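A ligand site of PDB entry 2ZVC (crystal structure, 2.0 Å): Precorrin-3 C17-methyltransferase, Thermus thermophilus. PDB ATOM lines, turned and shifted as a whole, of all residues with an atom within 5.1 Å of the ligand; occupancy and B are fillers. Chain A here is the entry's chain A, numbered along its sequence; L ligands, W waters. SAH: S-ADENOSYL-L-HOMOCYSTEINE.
The backbone carbonyl oxygen (O) of Thr 239 sits at hydrogen-bond distance from an oxygen (O2') of the ligand (2.6 Å). O of Met 237 is in hydrogen-bond range of O3' of the ligand, at 2.6 Å. N3 of the ligand sits at hydrogen-bond distance from OG1 of Thr 240, 2.6 Å away. The backbone carbonyl oxygen (O) of Ile 87 sits at hydrogen-bond distance from a nitrogen (N) of the ligand (2.6 Å). O of the ligand lies within hydrogen-bond range of OG1 of Thr 132. O of the ligand sits at hydrogen-bond distance from N of Asp 84, 2.8 Å away. The backbone carbonyl oxygen of Asp 84 sits at hydrogen-bond distance from a nitrogen (N) of the ligand. The backbone carbonyl oxygen (O) of Gly 82 is in hydrogen-bond range of a nitrogen (N) of the ligand, 2.9 Å away. The backbone NH (N) of Ala 215 lies within hydrogen-bond range of a nitrogen (N1) of the ligand (2.9 Å). O of Ala 215 is in hydrogen-bond range of N6 of the ligand (3.0 Å). OXT of the ligand sits at hydrogen-bond distance from N of Ala 133 (3.0 Å). O of Pro 11 sits at hydrogen-bond distance from N6 of the ligand. An oxygen (O2') of the ligand is in hydrogen-bond range of the backbone NH of Asn 182, 3.1 Å away. The side-chain amide nitrogen of Asn 182 sits close to a sulfur (SD) of the ligand (3.3 Å).
The side-chain hydroxyl of Thr 239 lies within hydrogen-bond range of the backbone NH of Gly 236, 3.3 Å away. The backbone NH (N) of Val 212 sits at hydrogen-bond distance from the backbone carbonyl oxygen (O) of Thr 240 (3.0 Å). The side-chain hydroxyl (OG1) of Thr 132 sits at hydrogen-bond distance from the side-chain hydroxyl (OH) of Tyr 181, at 2.6 Å. O of Pro 11 is in hydrogen-bond range of NE of Arg 217 (2.7 Å). The backbone carbonyl oxygen of Leu 238 sits at hydrogen-bond distance from the backbone NH of Ser 214 (2.9 Å).
The guanidinium group (NE) of Arg 217 sits close to a nitrogen (N6) of the ligand. Gly 83 touches the ligand (CA to O, 3.5 Å). O of Tyr 88 touches CG of the ligand (3.4 Å). Tyr 181 touches the ligand. Pro 183 touches the ligand. Val 212 touches the ligand. N of Ser 214 touches N1 of the ligand (3.7 Å). Leu 238 touches the ligand. The nearest printed residue that does not touch the ligand is Val 137 (4.02 Å).
Water W4 lies within hydrogen-bond range of N of the ligand, OH of Tyr 37 and N of Gly 82. Water W3 lies within hydrogen-bond range of the guanidinium group (NH2) of Arg 217 (2.7 Å), a nitrogen (N7) of the ligand (3.0 Å), the backbone carbonyl oxygen (O) of Pro 11 (3.3 Å) and the backbone NH (N) of Gly 83 (3.4 Å). Water W1 lies within hydrogen-bond range of the side-chain amide nitrogen (ND2) of Asn 182 and an oxygen (O3') of the ligand.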
ATOM      1  N   PRO A  11      -7.056  16.744  -3.257  1.00  0.00           N
ATOM      2  CA  PRO A  11      -6.460  17.246  -4.498  1.00  0.00           C
ATOM      3  C   PRO A  11      -6.543  16.365  -5.739  1.00  0.00           C
ATOM      4  O   PRO A  11      -6.525  16.873  -6.860  1.00  0.00           O
ATOM      5  CB  PRO A  11      -5.029  17.570  -4.092  1.00  0.00           C
ATOM      6  CG  PRO A  11      -4.741  16.557  -3.038  1.00  0.00           C
ATOM      7  CD  PRO A  11      -6.016  16.548  -2.229  1.00  0.00           C
ATOM      8  N   GLY A  12      -6.623  15.047  -5.555  1.00  0.00           N
ATOM      9  CA  GLY A  12      -6.727  14.185  -6.727  1.00  0.00           C
ATOM     10  C   GLY A  12      -5.936  12.898  -6.754  1.00  0.00           C
ATOM     11  O   GLY A  12      -6.111  12.103  -7.674  1.00  0.00           O
ATOM     12  N   TYR A  37     -13.458  14.142 -11.960  1.00  0.00           N
ATOM     13  CA  TYR A  37     -13.310  13.520 -10.644  1.00  0.00           C
ATOM     14  C   TYR A  37     -13.613  12.024 -10.710  1.00  0.00           C
ATOM     15  O   TYR A  37     -12.887  11.208 -10.135  1.00  0.00           O
ATOM     16  CB  TYR A  37     -14.259  14.166  -9.609  1.00  0.00           C
ATOM     17  CG  TYR A  37     -14.158  15.677  -9.476  1.00  0.00           C
ATOM     18  CD1 TYR A  37     -12.930  16.334  -9.566  1.00  0.00           C
ATOM     19  CD2 TYR A  37     -15.297  16.429  -9.200  1.00  0.00           C
ATOM     20  CE1 TYR A  37     -12.847  17.723  -9.375  1.00  0.00           C
ATOM     21  CE2 TYR A  37     -15.222  17.807  -9.006  1.00  0.00           C
ATOM     22  CZ  TYR A  37     -14.002  18.453  -9.092  1.00  0.00           C
ATOM     23  OH  TYR A  37     -13.943  19.809  -8.891  1.00  0.00           O
ATOM     24  N   SER A  81     -16.825  15.516  -4.942  1.00  0.00           N
ATOM     25  CA  SER A  81     -16.351  16.864  -5.240  1.00  0.00           C
ATOM     26  C   SER A  81     -14.840  16.841  -5.037  1.00  0.00           C
ATOM     27  O   SER A  81     -14.344  16.175  -4.120  1.00  0.00           O
ATOM     28  CB  SER A  81     -16.932  17.902  -4.262  1.00  0.00           C
ATOM     29  OG  SER A  81     -18.308  18.175  -4.507  1.00  0.00           O
ATOM     30  N   GLY A  82     -14.094  17.525  -5.897  1.00  0.00           N
ATOM     31  CA  GLY A  82     -12.653  17.572  -5.718  1.00  0.00           C
ATOM     32  C   GLY A  82     -12.448  18.360  -4.437  1.00  0.00           C
ATOM     33  O   GLY A  82     -13.308  19.151  -4.078  1.00  0.00           O
ATOM     34  N   GLY A  83     -11.332  18.144  -3.750  1.00  0.00           N
ATOM     35  CA  GLY A  83     -11.073  18.877  -2.515  1.00  0.00           C
ATOM     36  C   GLY A  83     -12.124  18.643  -1.447  1.00  0.00           C
ATOM     37  O   GLY A  83     -12.291  17.512  -0.983  1.00  0.00           O
ATOM     38  N   ASP A  84     -12.824  19.699  -1.054  1.00  0.00           N
ATOM     39  CA  ASP A  84     -13.880  19.614  -0.038  1.00  0.00           C
ATOM     40  C   ASP A  84     -15.215  20.013  -0.676  1.00  0.00           C
ATOM     41  O   ASP A  84     -15.273  20.964  -1.454  1.00  0.00           O
ATOM     42  CB  ASP A  84     -13.583  20.562   1.137  1.00  0.00           C
ATOM     43  CG  ASP A  84     -14.510  20.337   2.321  1.00  0.00           C
ATOM     44  OD1 ASP A  84     -15.621  20.915   2.336  1.00  0.00           O
ATOM     45  OD2 ASP A  84     -14.131  19.564   3.232  1.00  0.00           O
ATOM     46  N   PRO A  85     -16.319  19.298  -0.338  1.00  0.00           N
ATOM     47  CA  PRO A  85     -17.633  19.611  -0.913  1.00  0.00           C
ATOM     48  C   PRO A  85     -18.182  20.990  -0.520  1.00  0.00           C
ATOM     49  O   PRO A  85     -19.007  21.557  -1.225  1.00  0.00           O
ATOM     50  CB  PRO A  85     -18.530  18.485  -0.373  1.00  0.00           C
ATOM     51  CG  PRO A  85     -17.556  17.362  -0.060  1.00  0.00           C
ATOM     52  CD  PRO A  85     -16.399  18.119   0.545  1.00  0.00           C
ATOM     53  N   ILE A  87     -16.446  23.804  -0.300  1.00  0.00           N
ATOM     54  CA  ILE A  87     -15.666  24.904  -0.851  1.00  0.00           C
ATOM     55  C   ILE A  87     -15.870  24.928  -2.360  1.00  0.00           C
ATOM     56  O   ILE A  87     -15.214  24.199  -3.100  1.00  0.00           O
ATOM     57  CB  ILE A  87     -14.153  24.722  -0.543  1.00  0.00           C
ATOM     58  CG1 ILE A  87     -13.938  24.639   0.976  1.00  0.00           C
ATOM     59  CG2 ILE A  87     -13.358  25.894  -1.116  1.00  0.00           C
ATOM     60  CD1 ILE A  87     -14.447  25.841   1.728  1.00  0.00           C
ATOM     61  N   TYR A  88     -16.797  25.771  -2.796  1.00  0.00           N
ATOM     62  CA  TYR A  88     -17.134  25.910  -4.215  1.00  0.00           C
ATOM     63  C   TYR A  88     -17.441  24.503  -4.752  1.00  0.00           C
ATOM     64  O   TYR A  88     -17.066  24.140  -5.867  1.00  0.00           O
ATOM     65  CB  TYR A  88     -15.960  26.533  -4.971  1.00  0.00           C
ATOM     66  CG  TYR A  88     -15.453  27.829  -4.356  1.00  0.00           C
ATOM     67  CD1 TYR A  88     -16.299  28.930  -4.214  1.00  0.00           C
ATOM     68  CD2 TYR A  88     -14.146  27.936  -3.894  1.00  0.00           C
ATOM     69  CE1 TYR A  88     -15.850  30.116  -3.625  1.00  0.00           C
ATOM     70  CE2 TYR A  88     -13.688  29.123  -3.307  1.00  0.00           C
ATOM     71  CZ  TYR A  88     -14.544  30.203  -3.171  1.00  0.00           C
ATOM     72  OH  TYR A  88     -14.100  31.377  -2.600  1.00  0.00           O
ATOM     73  N   GLY A  89     -18.129  23.715  -3.915  1.00  0.00           N
ATOM     74  CA  GLY A  89     -18.464  22.338  -4.275  1.00  0.00           C
ATOM     75  C   GLY A  89     -19.943  22.017  -4.326  1.00  0.00           C
ATOM     76  O   GLY A  89     -20.780  22.887  -4.552  1.00  0.00           O
ATOM     77  N   VAL A 131      -9.220  17.657   1.888  1.00  0.00           N
ATOM     78  CA  VAL A 131      -8.197  18.701   1.808  1.00  0.00           C
ATOM     79  C   VAL A 131      -8.575  19.619   0.643  1.00  0.00           C
ATOM     80  O   VAL A 131      -8.596  19.182  -0.503  1.00  0.00           O
ATOM     81  CB  VAL A 131      -6.803  18.095   1.552  1.00  0.00           C
ATOM     82  CG1 VAL A 131      -5.772  19.197   1.360  1.00  0.00           C
ATOM     83  CG2 VAL A 131      -6.402  17.200   2.729  1.00  0.00           C
ATOM     84  N   THR A 132      -8.876  20.878   0.940  1.00  0.00           N
ATOM     85  CA  THR A 132      -9.262  21.808  -0.118  1.00  0.00           C
ATOM     86  C   THR A 132      -8.022  22.299  -0.855  1.00  0.00           C
ATOM     87  O   THR A 132      -6.907  22.200  -0.344  1.00  0.00           O
ATOM     88  CB  THR A 132     -10.094  23.002   0.436  1.00  0.00           C
ATOM     89  OG1 THR A 132     -10.648  23.737  -0.656  1.00  0.00           O
ATOM     90  CG2 THR A 132      -9.226  23.929   1.284  1.00  0.00           C
ATOM     91  N   ALA A 133      -8.220  22.816  -2.073  1.00  0.00           N
ATOM     92  CA  ALA A 133      -7.113  23.297  -2.891  1.00  0.00           C
ATOM     93  C   ALA A 133      -6.136  24.214  -2.164  1.00  0.00           C
ATOM     94  O   ALA A 133      -4.923  24.081  -2.308  1.00  0.00           O
ATOM     95  CB  ALA A 133      -7.658  23.998  -4.153  1.00  0.00           C
ATOM     96  N   VAL A 137      -2.302  23.104  -2.199  1.00  0.00           N
ATOM     97  CA  VAL A 137      -1.256  23.822  -2.919  1.00  0.00           C
ATOM     98  C   VAL A 137      -0.265  24.465  -1.944  1.00  0.00           C
ATOM     99  O   VAL A 137       0.927  24.548  -2.224  1.00  0.00           O
ATOM    100  CB  VAL A 137      -1.847  24.888  -3.875  1.00  0.00           C
ATOM    101  CG1 VAL A 137      -2.917  24.247  -4.770  1.00  0.00           C
ATOM    102  CG2 VAL A 137      -2.419  26.053  -3.100  1.00  0.00           C
ATOM    103  N   LEU A 180      -6.794  32.292  -4.834  1.00  0.00           N
ATOM    104  CA  LEU A 180      -7.792  32.413  -5.893  1.00  0.00           C
ATOM    105  C   LEU A 180      -8.190  31.062  -6.487  1.00  0.00           C
ATOM    106  O   LEU A 180      -7.374  30.369  -7.093  1.00  0.00           O
ATOM    107  CB  LEU A 180      -7.269  33.322  -7.011  1.00  0.00           C
ATOM    108  CG  LEU A 180      -6.936  34.761  -6.601  1.00  0.00           C
ATOM    109  CD1 LEU A 180      -6.409  35.537  -7.817  1.00  0.00           C
ATOM    110  CD2 LEU A 180      -8.174  35.437  -6.022  1.00  0.00           C
ATOM    111  N   TYR A 181      -9.453  30.695  -6.301  1.00  0.00           N
ATOM    112  CA  TYR A 181     -10.000  29.457  -6.854  1.00  0.00           C
ATOM    113  C   TYR A 181     -10.601  29.814  -8.221  1.00  0.00           C
ATOM    114  O   TYR A 181     -11.043  30.951  -8.408  1.00  0.00           O
ATOM    115  CB  TYR A 181     -11.110  28.896  -5.955  1.00  0.00           C
ATOM    116  CG  TYR A 181     -10.647  28.112  -4.743  1.00  0.00           C
ATOM    117  CD1 TYR A 181     -10.105  28.769  -3.640  1.00  0.00           C
ATOM    118  CD2 TYR A 181     -10.821  26.728  -4.671  1.00  0.00           C
ATOM    119  CE1 TYR A 181      -9.745  28.060  -2.484  1.00  0.00           C
ATOM    120  CE2 TYR A 181     -10.460  26.009  -3.514  1.00  0.00           C
ATOM    121  CZ  TYR A 181      -9.937  26.694  -2.428  1.00  0.00           C
ATOM    122  OH  TYR A 181      -9.624  25.999  -1.278  1.00  0.00           O
ATOM    123  N   ASN A 182     -10.622  28.869  -9.151  1.00  0.00           N
ATOM    124  CA  ASN A 182     -11.187  29.121 -10.481  1.00  0.00           C
ATOM    125  C   ASN A 182     -10.601  30.428 -11.024  1.00  0.00           C
ATOM    126  O   ASN A 182     -11.340  31.296 -11.462  1.00  0.00           O
ATOM    127  CB  ASN A 182     -12.708  29.262 -10.392  1.00  0.00           C
ATOM    128  CG  ASN A 182     -13.363  28.156  -9.575  1.00  0.00           C
ATOM    129  OD1 ASN A 182     -13.984  28.422  -8.529  1.00  0.00           O
ATOM    130  ND2 ASN A 182     -13.240  26.929 -10.037  1.00  0.00           N
ATOM    131  N   PRO A 183      -9.271  30.546 -11.046  1.00  0.00           N
ATOM    132  CA  PRO A 183      -8.596  31.765 -11.518  1.00  0.00           C
ATOM    133  C   PRO A 183      -8.745  32.171 -12.977  1.00  0.00           C
ATOM    134  O   PRO A 183      -8.649  33.357 -13.285  1.00  0.00           O
ATOM    135  CB  PRO A 183      -7.140  31.496 -11.163  1.00  0.00           C
ATOM    136  CG  PRO A 183      -7.023  30.041 -11.416  1.00  0.00           C
ATOM    137  CD  PRO A 183      -8.295  29.472 -10.801  1.00  0.00           C
ATOM    138  N   VAL A 212      -0.112  27.204  -8.810  1.00  0.00           N
ATOM    139  CA  VAL A 212       0.093  25.782  -8.640  1.00  0.00           C
ATOM    140  C   VAL A 212      -0.964  25.054  -9.438  1.00  0.00           C
ATOM    141  O   VAL A 212      -2.164  25.172  -9.170  1.00  0.00           O
ATOM    142  CB  VAL A 212      -0.014  25.363  -7.157  1.00  0.00           C
ATOM    143  CG1 VAL A 212       0.241  23.856  -7.029  1.00  0.00           C
ATOM    144  CG2 VAL A 212       0.992  26.145  -6.335  1.00  0.00           C
ATOM    145  N   LYS A 213      -0.496  24.294 -10.429  1.00  0.00           N
ATOM    146  CA  LYS A 213      -1.362  23.558 -11.323  1.00  0.00           C
ATOM    147  C   LYS A 213      -1.377  22.070 -11.043  1.00  0.00           C
ATOM    148  O   LYS A 213      -0.333  21.471 -10.769  1.00  0.00           O
ATOM    149  CB  LYS A 213      -0.909  23.804 -12.761  1.00  0.00           C
ATOM    150  CG  LYS A 213      -1.527  22.856 -13.787  1.00  0.00           C
ATOM    151  CD  LYS A 213      -0.681  22.826 -15.052  1.00  0.00           C
ATOM    152  CE  LYS A 213      -1.059  21.662 -15.952  1.00  0.00           C
ATOM    153  NZ  LYS A 213      -0.101  21.519 -17.089  1.00  0.00           N
ATOM    154  N   SER A 214      -2.572  21.483 -11.107  1.00  0.00           N
ATOM    155  CA  SER A 214      -2.757  20.051 -10.900  1.00  0.00           C
ATOM    156  C   SER A 214      -1.980  19.520  -9.707  1.00  0.00           C
ATOM    157  O   SER A 214      -1.216  18.550  -9.820  1.00  0.00           O
ATOM    158  CB  SER A 214      -2.325  19.279 -12.153  1.00  0.00           C
ATOM    159  OG  SER A 214      -3.066  19.715 -13.278  1.00  0.00           O
ATOM    160  N   ALA A 215      -2.174  20.150  -8.555  1.00  0.00           N
ATOM    161  CA  ALA A 215      -1.498  19.728  -7.335  1.00  0.00           C
ATOM    162  C   ALA A 215      -1.799  18.261  -7.045  1.00  0.00           C
ATOM    163  O   ALA A 215      -2.966  17.852  -7.057  1.00  0.00           O
ATOM    164  CB  ALA A 215      -1.926  20.609  -6.155  1.00  0.00           C
ATOM    165  N   ARG A 217      -1.382  15.737  -8.856  1.00  0.00           N
ATOM    166  CA  ARG A 217      -1.866  14.996 -10.004  1.00  0.00           C
ATOM    167  C   ARG A 217      -0.786  14.922 -11.070  1.00  0.00           C
ATOM    168  O   ARG A 217       0.319  15.449 -10.886  1.00  0.00           O
ATOM    169  CB  ARG A 217      -3.107  15.671 -10.608  1.00  0.00           C
ATOM    170  CG  ARG A 217      -4.277  15.841  -9.646  1.00  0.00           C
ATOM    171  CD  ARG A 217      -5.519  16.250 -10.410  1.00  0.00           C
ATOM    172  NE  ARG A 217      -6.562  16.798  -9.559  1.00  0.00           N
ATOM    173  CZ  ARG A 217      -7.748  17.212 -10.005  1.00  0.00           C
ATOM    174  NH1 ARG A 217      -8.026  17.141 -11.302  1.00  0.00           N
ATOM    175  NH2 ARG A 217      -8.631  17.731  -9.164  1.00  0.00           N
ATOM    176  N   GLY A 236      -5.159  28.196 -15.548  1.00  0.00           N
ATOM    177  CA  GLY A 236      -6.221  27.372 -16.116  1.00  0.00           C
ATOM    178  C   GLY A 236      -7.221  26.972 -15.054  1.00  0.00           C
ATOM    179  O   GLY A 236      -7.197  27.479 -13.935  1.00  0.00           O
ATOM    180  N   MET A 237      -8.111  26.046 -15.408  1.00  0.00           N
ATOM    181  CA  MET A 237      -9.116  25.603 -14.436  1.00  0.00           C
ATOM    182  C   MET A 237      -8.550  24.585 -13.443  1.00  0.00           C
ATOM    183  O   MET A 237      -9.170  24.203 -12.478  1.00  0.00           O
ATOM    184  CB  MET A 237     -10.350  25.034 -15.165  1.00  0.00           C
ATOM    185  CG  MET A 237     -10.011  24.309 -16.485  1.00  0.00           C
ATOM    186  SD  MET A 237     -11.489  23.943 -17.443  1.00  0.00           S
ATOM    187  CE  MET A 237     -11.672  25.544 -18.225  1.00  0.00           C
ATOM    188  N   LEU A 238      -7.321  24.116 -13.759  1.00  0.00           N
ATOM    189  CA  LEU A 238      -6.622  23.215 -12.830  1.00  0.00           C
ATOM    190  C   LEU A 238      -5.584  23.972 -11.985  1.00  0.00           C
ATOM    191  O   LEU A 238      -4.697  23.391 -11.386  1.00  0.00           O
ATOM    192  CB  LEU A 238      -5.900  22.141 -13.631  1.00  0.00           C
ATOM    193  CG  LEU A 238      -6.835  21.197 -14.402  1.00  0.00           C
ATOM    194  CD1 LEU A 238      -6.055  20.160 -15.235  1.00  0.00           C
ATOM    195  CD2 LEU A 238      -7.751  20.371 -13.496  1.00  0.00           C
ATOM    196  N   THR A 239      -5.704  25.319 -11.967  1.00  0.00           N
ATOM    197  CA  THR A 239      -4.729  26.135 -11.253  1.00  0.00           C
ATOM    198  C   THR A 239      -5.353  26.879 -10.071  1.00  0.00           C
ATOM    199  O   THR A 239      -6.481  27.342 -10.116  1.00  0.00           O
ATOM    200  CB  THR A 239      -4.152  27.166 -12.229  1.00  0.00           C
ATOM    201  OG1 THR A 239      -3.434  26.489 -13.268  1.00  0.00           O
ATOM    202  CG2 THR A 239      -3.193  28.102 -11.486  1.00  0.00           C
ATOM    203  N   THR A 240      -4.555  26.994  -9.015  1.00  0.00           N
ATOM    204  CA  THR A 240      -4.936  27.761  -7.831  1.00  0.00           C
ATOM    205  C   THR A 240      -3.817  28.793  -7.699  1.00  0.00           C
ATOM    206  O   THR A 240      -2.630  28.455  -7.810  1.00  0.00           O
ATOM    207  CB  THR A 240      -4.993  26.909  -6.546  1.00  0.00           C
ATOM    208  OG1 THR A 240      -6.062  25.975  -6.649  1.00  0.00           O
ATOM    209  CG2 THR A 240      -5.213  27.789  -5.319  1.00  0.00           C
HETATM  210  N   SAH L   1     -14.267  21.835  -3.810  1.00  0.00           N
HETATM  211  CA  SAH L   1     -12.932  22.118  -4.500  1.00  0.00           C
HETATM  212  CB  SAH L   1     -12.888  23.281  -5.433  1.00  0.00           C
HETATM  213  CG  SAH L   1     -13.858  23.302  -6.600  1.00  0.00           C
HETATM  214  SD  SAH L   1     -13.475  24.812  -7.565  1.00  0.00           S
HETATM  215  C   SAH L   1     -11.855  22.293  -3.352  1.00  0.00           C
HETATM  216  O   SAH L   1     -12.208  22.196  -2.158  1.00  0.00           O
HETATM  217  OXT SAH L   1     -10.644  22.517  -3.743  1.00  0.00           O
HETATM  218  C5' SAH L   1     -12.280  24.186  -8.683  1.00  0.00           C
HETATM  219  C4' SAH L   1     -10.949  25.026  -8.503  1.00  0.00           C
HETATM  220  O4' SAH L   1     -10.293  24.561  -7.295  1.00  0.00           O
HETATM  221  C3' SAH L   1      -9.933  24.903  -9.586  1.00  0.00           C
HETATM  222  O3' SAH L   1     -10.245  25.781 -10.665  1.00  0.00           O
HETATM  223  C2' SAH L   1      -8.643  25.248  -8.807  1.00  0.00           C
HETATM  224  O2' SAH L   1      -8.497  26.665  -8.640  1.00  0.00           O
HETATM  225  C1' SAH L   1      -8.803  24.504  -7.474  1.00  0.00           C
HETATM  226  N9  SAH L   1      -8.367  23.211  -7.454  1.00  0.00           N
HETATM  227  C8  SAH L   1      -8.988  22.003  -7.223  1.00  0.00           C
HETATM  228  N7  SAH L   1      -8.213  20.955  -7.271  1.00  0.00           N
HETATM  229  C5  SAH L   1      -6.924  21.484  -7.573  1.00  0.00           C
HETATM  230  C6  SAH L   1      -5.635  20.836  -7.748  1.00  0.00           C
HETATM  231  N6  SAH L   1      -5.437  19.512  -7.657  1.00  0.00           N
HETATM  232  N1  SAH L   1      -4.595  21.695  -8.032  1.00  0.00           N
HETATM  233  C2  SAH L   1      -4.739  23.045  -8.143  1.00  0.00           C
HETATM  234  N3  SAH L   1      -5.942  23.696  -7.965  1.00  0.00           N
HETATM  235  C4  SAH L   1      -6.988  22.855  -7.691  1.00  0.00           C
HETATM  236  O   HOH W   1     -12.782  26.327 -12.632  1.00  0.00           O
HETATM  237  O   HOH W   2     -11.780  20.647  -7.658  1.00  0.00           O
HETATM  238  O   HOH W   3      -9.510  18.344  -6.639  1.00  0.00           O
HETATM  239  O   HOH W   4     -15.451  20.534  -6.205  1.00  0.00           O
